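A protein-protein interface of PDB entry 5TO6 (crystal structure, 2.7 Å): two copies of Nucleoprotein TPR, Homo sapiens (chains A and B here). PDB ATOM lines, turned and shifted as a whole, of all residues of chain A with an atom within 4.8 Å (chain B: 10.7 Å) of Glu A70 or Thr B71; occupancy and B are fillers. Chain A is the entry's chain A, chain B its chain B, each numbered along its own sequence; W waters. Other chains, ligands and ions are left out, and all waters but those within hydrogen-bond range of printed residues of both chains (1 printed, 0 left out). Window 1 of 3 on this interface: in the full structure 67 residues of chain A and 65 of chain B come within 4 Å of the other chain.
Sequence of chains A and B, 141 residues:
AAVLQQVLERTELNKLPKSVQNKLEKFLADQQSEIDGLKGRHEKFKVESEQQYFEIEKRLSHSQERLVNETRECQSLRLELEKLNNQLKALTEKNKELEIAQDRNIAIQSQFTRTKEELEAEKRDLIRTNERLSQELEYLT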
ATOM      1  N   ARG A  66      30.383 -18.734 -19.591  1.00  0.00           N
ATOM      2  CA  ARG A  66      29.582 -17.622 -19.100  1.00  0.00           C
ATOM      3  C   ARG A  66      30.402 -16.654 -18.248  1.00  0.00           C
ATOM      4  O   ARG A  66      30.226 -15.438 -18.335  1.00  0.00           O
ATOM      5  CB  ARG A  66      28.398 -18.160 -18.295  1.00  0.00           C
ATOM      6  CG  ARG A  66      27.331 -18.816 -19.152  1.00  0.00           C
ATOM      7  CD  ARG A  66      26.271 -19.496 -18.301  1.00  0.00           C
ATOM      8  NE  ARG A  66      25.052 -19.776 -19.054  1.00  0.00           N
ATOM      9  CZ  ARG A  66      23.946 -20.288 -18.522  1.00  0.00           C
ATOM     10  NH1 ARG A  66      23.908 -20.588 -17.231  1.00  0.00           N
ATOM     11  NH2 ARG A  66      22.884 -20.513 -19.282  1.00  0.00           N
ATOM     12  N   LEU A  67      31.291 -17.203 -17.425  1.00  0.00           N
ATOM     13  CA  LEU A  67      32.153 -16.396 -16.566  1.00  0.00           C
ATOM     14  C   LEU A  67      33.161 -15.582 -17.369  1.00  0.00           C
ATOM     15  O   LEU A  67      33.376 -14.401 -17.100  1.00  0.00           O
ATOM     16  CB  LEU A  67      32.887 -17.283 -15.560  1.00  0.00           C
ATOM     17  CG  LEU A  67      33.874 -16.562 -14.640  1.00  0.00           C
ATOM     18  CD1 LEU A  67      33.165 -15.510 -13.801  1.00  0.00           C
ATOM     19  CD2 LEU A  67      34.600 -17.556 -13.752  1.00  0.00           C
ATOM     20  N   VAL A  68      33.778 -16.224 -18.357  1.00  0.00           N
ATOM     21  CA  VAL A  68      34.794 -15.578 -19.177  1.00  0.00           C
ATOM     22  C   VAL A  68      34.187 -14.440 -19.995  1.00  0.00           C
ATOM     23  O   VAL A  68      34.799 -13.381 -20.158  1.00  0.00           O
ATOM     24  CB  VAL A  68      35.474 -16.606 -20.116  1.00  0.00           C
ATOM     25  CG1 VAL A  68      36.054 -15.933 -21.350  1.00  0.00           C
ATOM     26  CG2 VAL A  68      36.548 -17.384 -19.366  1.00  0.00           C
ATOM     27  N   ASN A  69      32.964 -14.647 -20.470  1.00  0.00           N
ATOM     28  CA  ASN A  69      32.249 -13.621 -21.217  1.00  0.00           C
ATOM     29  C   ASN A  69      31.903 -12.424 -20.344  1.00  0.00           C
ATOM     30  O   ASN A  69      32.161 -11.279 -20.716  1.00  0.00           O
ATOM     31  CB  ASN A  69      30.983 -14.204 -21.843  1.00  0.00           C
ATOM     32  CG  ASN A  69      31.288 -15.167 -22.971  1.00  0.00           C
ATOM     33  OD1 ASN A  69      32.399 -15.184 -23.500  1.00  0.00           O
ATOM     34  ND2 ASN A  69      30.303 -15.974 -23.345  1.00  0.00           N
ATOM     35  N   GLU A  70      31.309 -12.697 -19.187  1.00  0.00           N
ATOM     36  CA  GLU A  70      30.936 -11.646 -18.251  1.00  0.00           C
ATOM     37  C   GLU A  70      32.163 -10.867 -17.801  1.00  0.00           C
ATOM     38  O   GLU A  70      32.113  -9.649 -17.652  1.00  0.00           O
ATOM     39  CB  GLU A  70      30.211 -12.232 -17.038  1.00  0.00           C
ATOM     40  CG  GLU A  70      29.563 -11.183 -16.151  1.00  0.00           C
ATOM     41  CD  GLU A  70      28.408 -10.477 -16.831  1.00  0.00           C
ATOM     42  OE1 GLU A  70      27.833 -11.047 -17.782  1.00  0.00           O
ATOM     43  OE2 GLU A  70      28.078  -9.343 -16.422  1.00  0.00           O
ATOM     44  N   THR A  71      33.261 -11.582 -17.581  1.00  0.00           N
ATOM     45  CA  THR A  71      34.516 -10.958 -17.178  1.00  0.00           C
ATOM     46  C   THR A  71      35.035 -10.015 -18.261  1.00  0.00           C
ATOM     47  O   THR A  71      35.508  -8.921 -17.962  1.00  0.00           O
ATOM     48  CB  THR A  71      35.599 -12.016 -16.865  1.00  0.00           C
ATOM     49  OG1 THR A  71      35.121 -12.909 -15.851  1.00  0.00           O
ATOM     50  CG2 THR A  71      36.880 -11.352 -16.379  1.00  0.00           C
ATOM     51  N   ARG A  72      34.931 -10.435 -19.520  1.00  0.00           N
ATOM     52  CA  ARG A  72      35.422  -9.623 -20.629  1.00  0.00           C
ATOM     53  C   ARG A  72      34.588  -8.364 -20.830  1.00  0.00           C
ATOM     54  O   ARG A  72      35.135  -7.276 -21.014  1.00  0.00           O
ATOM     55  CB  ARG A  72      35.444 -10.437 -21.926  1.00  0.00           C
ATOM     56  CG  ARG A  72      35.984  -9.660 -23.121  1.00  0.00           C
ATOM     57  CD  ARG A  72      35.922 -10.465 -24.410  1.00  0.00           C
ATOM     58  NE  ARG A  72      34.564 -10.909 -24.716  1.00  0.00           N
ATOM     59  CZ  ARG A  72      34.153 -12.170 -24.630  1.00  0.00           C
ATOM     60  NH1 ARG A  72      34.999 -13.120 -24.251  1.00  0.00           N
ATOM     61  NH2 ARG A  72      32.898 -12.484 -24.925  1.00  0.00           N
ATOM     62  N   GLU A  73      33.265  -8.509 -20.803  1.00  0.00           N
ATOM     63  CA  GLU A  73      32.388  -7.349 -20.930  1.00  0.00           C
ATOM     64  C   GLU A  73      32.581  -6.397 -19.759  1.00  0.00           C
ATOM     65  O   GLU A  73      32.640  -5.188 -19.940  1.00  0.00           O
ATOM     66  CB  GLU A  73      30.918  -7.765 -21.025  1.00  0.00           C
ATOM     67  CG  GLU A  73      30.479  -8.220 -22.410  1.00  0.00           C
ATOM     68  CD  GLU A  73      28.977  -8.436 -22.503  1.00  0.00           C
ATOM     69  OE1 GLU A  73      28.295  -8.368 -21.457  1.00  0.00           O
ATOM     70  OE2 GLU A  73      28.475  -8.659 -23.625  1.00  0.00           O
ATOM     71  N   CYS A  74      32.700  -6.954 -18.560  1.00  0.00           N
ATOM     72  CA  CYS A  74      32.892  -6.148 -17.361  1.00  0.00           C
ATOM     73  C   CYS A  74      34.171  -5.329 -17.455  1.00  0.00           C
ATOM     74  O   CYS A  74      34.170  -4.142 -17.141  1.00  0.00           O
ATOM     75  CB  CYS A  74      32.922  -7.034 -16.113  1.00  0.00           C
ATOM     76  SG  CYS A  74      32.457  -6.184 -14.590  1.00  0.00           S
ATOM     77  N   SER B  63      32.974 -22.248 -10.102  1.00  0.00           N
ATOM     78  CA  SER B  63      32.749 -21.450 -11.300  1.00  0.00           C
ATOM     79  C   SER B  63      31.456 -20.650 -11.192  1.00  0.00           C
ATOM     80  O   SER B  63      31.407 -19.479 -11.568  1.00  0.00           O
ATOM     81  CB  SER B  63      32.717 -22.345 -12.539  1.00  0.00           C
ATOM     82  OG  SER B  63      32.516 -21.583 -13.716  1.00  0.00           O
ATOM     83  N   GLN B  64      30.411 -21.291 -10.676  1.00  0.00           N
ATOM     84  CA  GLN B  64      29.113 -20.646 -10.508  1.00  0.00           C
ATOM     85  C   GLN B  64      29.169 -19.477  -9.529  1.00  0.00           C
ATOM     86  O   GLN B  64      28.609 -18.414  -9.799  1.00  0.00           O
ATOM     87  CB  GLN B  64      28.066 -21.662 -10.046  1.00  0.00           C
ATOM     88  CG  GLN B  64      27.534 -22.547 -11.158  1.00  0.00           C
ATOM     89  CD  GLN B  64      26.786 -21.755 -12.218  1.00  0.00           C
ATOM     90  OE1 GLN B  64      27.183 -21.724 -13.382  1.00  0.00           O
ATOM     91  NE2 GLN B  64      25.695 -21.113 -11.816  1.00  0.00           N
ATOM     92  N   GLU B  65      29.837 -19.676  -8.395  1.00  0.00           N
ATOM     93  CA  GLU B  65      29.959 -18.624  -7.392  1.00  0.00           C
ATOM     94  C   GLU B  65      30.696 -17.404  -7.940  1.00  0.00           C
ATOM     95  O   GLU B  65      30.316 -16.268  -7.661  1.00  0.00           O
ATOM     96  CB  GLU B  65      30.668 -19.145  -6.141  1.00  0.00           C
ATOM     97  CG  GLU B  65      30.781 -18.111  -5.029  1.00  0.00           C
ATOM     98  CD  GLU B  65      31.532 -18.629  -3.819  1.00  0.00           C
ATOM     99  OE1 GLU B  65      32.714 -18.999  -3.969  1.00  0.00           O
ATOM    100  OE2 GLU B  65      30.940 -18.668  -2.720  1.00  0.00           O
ATOM    101  N   ARG B  66      31.745 -17.642  -8.722  1.00  0.00           N
ATOM    102  CA  ARG B  66      32.505 -16.549  -9.318  1.00  0.00           C
ATOM    103  C   ARG B  66      31.651 -15.785 -10.322  1.00  0.00           C
ATOM    104  O   ARG B  66      31.729 -14.559 -10.411  1.00  0.00           O
ATOM    105  CB  ARG B  66      33.771 -17.072  -9.998  1.00  0.00           C
ATOM    106  CG  ARG B  66      34.915 -17.367  -9.050  1.00  0.00           C
ATOM    107  CD  ARG B  66      36.202 -17.608  -9.817  1.00  0.00           C
ATOM    108  NE  ARG B  66      36.620 -16.429 -10.573  1.00  0.00           N
ATOM    109  CZ  ARG B  66      37.677 -16.396 -11.379  1.00  0.00           C
ATOM    110  NH1 ARG B  66      38.423 -17.482 -11.537  1.00  0.00           N
ATOM    111  NH2 ARG B  66      37.989 -15.281 -12.028  1.00  0.00           N
ATOM    112  N   LEU B  67      30.835 -16.519 -11.073  1.00  0.00           N
ATOM    113  CA  LEU B  67      29.967 -15.912 -12.075  1.00  0.00           C
ATOM    114  C   LEU B  67      28.917 -15.006 -11.437  1.00  0.00           C
ATOM    115  O   LEU B  67      28.675 -13.896 -11.912  1.00  0.00           O
ATOM    116  CB  LEU B  67      29.283 -16.993 -12.914  1.00  0.00           C
ATOM    117  CG  LEU B  67      28.255 -16.503 -13.937  1.00  0.00           C
ATOM    118  CD1 LEU B  67      28.881 -15.506 -14.906  1.00  0.00           C
ATOM    119  CD2 LEU B  67      27.635 -17.674 -14.692  1.00  0.00           C
ATOM    120  N   VAL B  68      28.293 -15.489 -10.367  1.00  0.00           N
ATOM    121  CA  VAL B  68      27.264 -14.727  -9.670  1.00  0.00           C
ATOM    122  C   VAL B  68      27.837 -13.442  -9.071  1.00  0.00           C
ATOM    123  O   VAL B  68      27.229 -12.377  -9.179  1.00  0.00           O
ATOM    124  CB  VAL B  68      26.601 -15.566  -8.557  1.00  0.00           C
ATOM    125  CG1 VAL B  68      25.628 -14.721  -7.754  1.00  0.00           C
ATOM    126  CG2 VAL B  68      25.892 -16.771  -9.160  1.00  0.00           C
ATOM    127  N   ASN B  69      29.010 -13.543  -8.454  1.00  0.00           N
ATOM    128  CA  ASN B  69      29.669 -12.372  -7.882  1.00  0.00           C
ATOM    129  C   ASN B  69      30.118 -11.368  -8.944  1.00  0.00           C
ATOM    130  O   ASN B  69      29.943 -10.162  -8.776  1.00  0.00           O
ATOM    131  CB  ASN B  69      30.862 -12.795  -7.022  1.00  0.00           C
ATOM    132  CG  ASN B  69      30.438 -13.471  -5.730  1.00  0.00           C
ATOM    133  OD1 ASN B  69      29.276 -13.391  -5.328  1.00  0.00           O
ATOM    134  ND2 ASN B  69      31.383 -14.129  -5.067  1.00  0.00           N
ATOM    135  N   GLU B  70      30.700 -11.863 -10.032  1.00  0.00           N
ATOM    136  CA  GLU B  70      31.145 -10.997 -11.121  1.00  0.00           C
ATOM    137  C   GLU B  70      29.981 -10.273 -11.791  1.00  0.00           C
ATOM    138  O   GLU B  70      30.106  -9.117 -12.191  1.00  0.00           O
ATOM    139  CB  GLU B  70      31.923 -11.804 -12.165  1.00  0.00           C
ATOM    140  CG  GLU B  70      32.590 -10.951 -13.230  1.00  0.00           C
ATOM    141  CD  GLU B  70      33.616  -9.989 -12.661  1.00  0.00           C
ATOM    142  OE1 GLU B  70      34.292 -10.345 -11.672  1.00  0.00           O
ATOM    143  OE2 GLU B  70      33.741  -8.870 -13.202  1.00  0.00           O
ATOM    144  N   THR B  71      28.851 -10.960 -11.905  1.00  0.00           N
ATOM    145  CA  THR B  71      27.655 -10.373 -12.494  1.00  0.00           C
ATOM    146  C   THR B  71      27.088  -9.249 -11.623  1.00  0.00           C
ATOM    147  O   THR B  71      26.643  -8.221 -12.138  1.00  0.00           O
ATOM    148  CB  THR B  71      26.565 -11.446 -12.717  1.00  0.00           C
ATOM    149  OG1 THR B  71      27.050 -12.444 -13.623  1.00  0.00           O
ATOM    150  CG2 THR B  71      25.296 -10.826 -13.286  1.00  0.00           C
ATOM    151  N   ARG B  72      27.109  -9.449 -10.307  1.00  0.00           N
ATOM    152  CA  ARG B  72      26.587  -8.468  -9.357  1.00  0.00           C
ATOM    153  C   ARG B  72      27.359  -7.145  -9.377  1.00  0.00           C
ATOM    154  O   ARG B  72      26.795  -6.079  -9.130  1.00  0.00           O
ATOM    155  CB  ARG B  72      26.598  -9.053  -7.941  1.00  0.00           C
ATOM    156  CG  ARG B  72      26.133  -8.083  -6.867  1.00  0.00           C
ATOM    157  CD  ARG B  72      26.203  -8.693  -5.483  1.00  0.00           C
ATOM    158  NE  ARG B  72      25.361  -9.879  -5.362  1.00  0.00           N
ATOM    159  CZ  ARG B  72      25.821 -11.104  -5.128  1.00  0.00           C
ATOM    160  NH1 ARG B  72      27.124 -11.311  -4.980  1.00  0.00           N
ATOM    161  NH2 ARG B  72      24.979 -12.123  -5.034  1.00  0.00           N
ATOM    162  N   GLU B  73      28.658  -7.217  -9.630  1.00  0.00           N
ATOM    163  CA  GLU B  73      29.477  -6.010  -9.701  1.00  0.00           C
ATOM    164  C   GLU B  73      29.374  -5.319 -11.062  1.00  0.00           C
ATOM    165  O   GLU B  73      29.425  -4.093 -11.152  1.00  0.00           O
ATOM    166  CB  GLU B  73      30.931  -6.348  -9.369  1.00  0.00           C
ATOM    167  CG  GLU B  73      31.056  -7.233  -8.134  1.00  0.00           C
ATOM    168  CD  GLU B  73      32.417  -7.152  -7.456  1.00  0.00           C
ATOM    169  OE1 GLU B  73      33.456  -7.303  -8.135  1.00  0.00           O
ATOM    170  OE2 GLU B  73      32.440  -6.951  -6.224  1.00  0.00           O
ATOM    171  N   CYS B  74      29.239  -6.120 -12.113  1.00  0.00           N
ATOM    172  CA  CYS B  74      29.073  -5.631 -13.482  1.00  0.00           C
ATOM    173  C   CYS B  74      27.732  -4.969 -13.822  1.00  0.00           C
ATOM    174  O   CYS B  74      27.679  -4.046 -14.638  1.00  0.00           O
ATOM    175  CB  CYS B  74      29.310  -6.785 -14.448  1.00  0.00           C
ATOM    176  SG  CYS B  74      30.704  -6.529 -15.547  1.00  0.00           S
ATOM    177  N   GLN B  75      26.657  -5.429 -13.194  1.00  0.00           N
ATOM    178  CA  GLN B  75      25.307  -4.976 -13.534  1.00  0.00           C
ATOM    179  C   GLN B  75      25.123  -3.455 -13.496  1.00  0.00           C
ATOM    180  O   GLN B  75      24.391  -2.889 -14.313  1.00  0.00           O
ATOM    181  CB  GLN B  75      24.295  -5.623 -12.583  1.00  0.00           C
ATOM    182  CG  GLN B  75      24.692  -5.479 -11.127  1.00  0.00           C
ATOM    183  CD  GLN B  75      23.522  -5.558 -10.158  1.00  0.00           C
ATOM    184  OE1 GLN B  75      22.411  -5.913 -10.542  1.00  0.00           O
ATOM    185  NE2 GLN B  75      23.769  -5.217  -8.894  1.00  0.00           N
ATOM    186  N   SER B  76      25.773  -2.810 -12.535  1.00  0.00           N
ATOM    187  CA  SER B  76      25.678  -1.367 -12.349  1.00  0.00           C
ATOM    188  C   SER B  76      26.327  -0.558 -13.472  1.00  0.00           C
ATOM    189  O   SER B  76      25.895   0.553 -13.769  1.00  0.00           O
ATOM    190  CB  SER B  76      26.313  -0.971 -11.014  1.00  0.00           C
ATOM    191  OG  SER B  76      27.682  -1.338 -10.981  1.00  0.00           O
ATOM    192  N   LEU B  77      27.358  -1.123 -14.093  1.00  0.00           N
ATOM    193  CA  LEU B  77      28.171  -0.400 -15.073  1.00  0.00           C
ATOM    194  C   LEU B  77      27.442   0.055 -16.339  1.00  0.00           C
ATOM    195  O   LEU B  77      27.658   1.178 -16.800  1.00  0.00           O
ATOM    196  CB  LEU B  77      29.375  -1.259 -15.472  1.00  0.00           C
ATOM    197  CG  LEU B  77      30.343  -1.605 -14.336  1.00  0.00           C
ATOM    198  CD1 LEU B  77      31.476  -2.492 -14.830  1.00  0.00           C
ATOM    199  CD2 LEU B  77      30.888  -0.343 -13.693  1.00  0.00           C
ATOM    200  N   ARG B  78      26.596  -0.800 -16.908  1.00  0.00           N
ATOM    201  CA  ARG B  78      25.882  -0.441 -18.131  1.00  0.00           C
ATOM    202  C   ARG B  78      24.955   0.754 -17.928  1.00  0.00           C
ATOM    203  O   ARG B  78      24.785   1.577 -18.829  1.00  0.00           O
ATOM    204  CB  ARG B  78      25.075  -1.629 -18.654  1.00  0.00           C
ATOM    205  CG  ARG B  78      25.883  -2.617 -19.469  1.00  0.00           C
ATOM    206  CD  ARG B  78      24.975  -3.630 -20.135  1.00  0.00           C
ATOM    207  NE  ARG B  78      25.540  -4.972 -20.081  1.00  0.00           N
ATOM    208  CZ  ARG B  78      25.378  -5.801 -19.056  1.00  0.00           C
ATOM    209  NH1 ARG B  78      24.666  -5.423 -18.003  1.00  0.00           N
ATOM    210  NH2 ARG B  78      25.925  -7.006 -19.085  1.00  0.00           N
ATOM    211  N   LEU B  79      24.355   0.839 -16.744  1.00  0.00           N
ATOM    212  CA  LEU B  79      23.464   1.945 -16.412  1.00  0.00           C
ATOM    213  C   LEU B  79      24.257   3.240 -16.290  1.00  0.00           C
ATOM    214  O   LEU B  79      23.847   4.289 -16.790  1.00  0.00           O
ATOM    215  CB  LEU B  79      22.723   1.680 -15.099  1.00  0.00           C
ATOM    216  CG  LEU B  79      21.621   2.688 -14.750  1.00  0.00           C
ATOM    217  CD1 LEU B  79      20.269   2.206 -15.258  1.00  0.00           C
ATOM    218  CD2 LEU B  79      21.575   3.054 -13.262  1.00  0.00           C
HETATM  219  O   HOH W   1      25.799 -21.879 -15.874  1.00  0.00           O
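The backbone carbonyl oxygen of Leu A67 is in hydrogen-bond range of the side-chain hydroxyl of Thr A71 (2.6 Å).
The backbone carbonyl oxygen (O) of Leu B67 is in hydrogen-bond range of the side-chain hydroxyl (OG1) of Thr B71.
Water W1 lies within hydrogen-bond range of NH1 of Arg A66 (2.7 Å) and OE1 of Gln B64 (2.9 Å).
Of the 9 printed residues of chain A, 5 touch a printed residue of chain B.
Of the 17 printed residues of chain B, 7 touch a printed residue of chain A.
Hydrophobic or aromatic side chains of chain B within 4 Å of the printed part of chain A: Leu B67 and Leu B77.
Among the printed residues, 9 pairs touch across the chains.
Leu A67 touches its own counterpart, Leu B67.
Glu A70 touches Thr B71, but with the chains exchanged Thr A71 does not touch Glu B70 (4.1 Å).
Glu A70 touches Cys B74, and with the chains exchanged Cys A74 touches Glu B70.
Cys B74 touches its own counterpart, Cys A74.
Of the 9 pairs that touch across the chains among the printed residues, 6 have their exchanged pair printed and touching as well.
OE1 of Glu A73 is in salt-bridge range of NH2 of Arg B78 (3.6 Å).
The side-chain sulfur (SG) of Cys B74 forms a disulfide with the side-chain sulfur (SG) of Cys A74 (2.0 Å).
The side-chain carboxylate (OE2) of Glu B70 lies close to the side-chain sulfur (SG) of Cys A74 (3.3 Å).
Printed residues of chain B within 4 Å of Leu A67: Arg B66 (3.8 Å) and Leu B67 (3.7 Å).
No residue of chain B comes within 4 Å of Asn A69.
Glu A70 touches just these residues of chain B: Thr B71 and Cys B74.
Thr A71 touches none of the printed residues of chain B.
Of chain B, only Arg B78 comes within 4 Å of Glu A73.
Cys A74 touches just these residues of chain B: Glu B70, Cys B74 and Leu B77.
Val B68 touches none of the printed residues of chain A.
Of chain A, only Glu A70 (3.8 Å) comes within 4 Å of Thr B71.
Printed residues of chain A within 4 Å of Leu B77: Cys A74.
Printed residues of chain A within 4 Å of Arg B78: Glu A73.
The nearest printed residue of chain A that does not touch Thr B71 is Arg A66 (6.4 Å).
Among the printed residues, pairs that only touch across the chains: Arg A66 with Leu B67, Leu A67 with Arg B66, Leu A67 with Leu B67, Glu A70 with Thr B71, Glu A70 with Cys B74 and Cys A74 with Leu B77.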
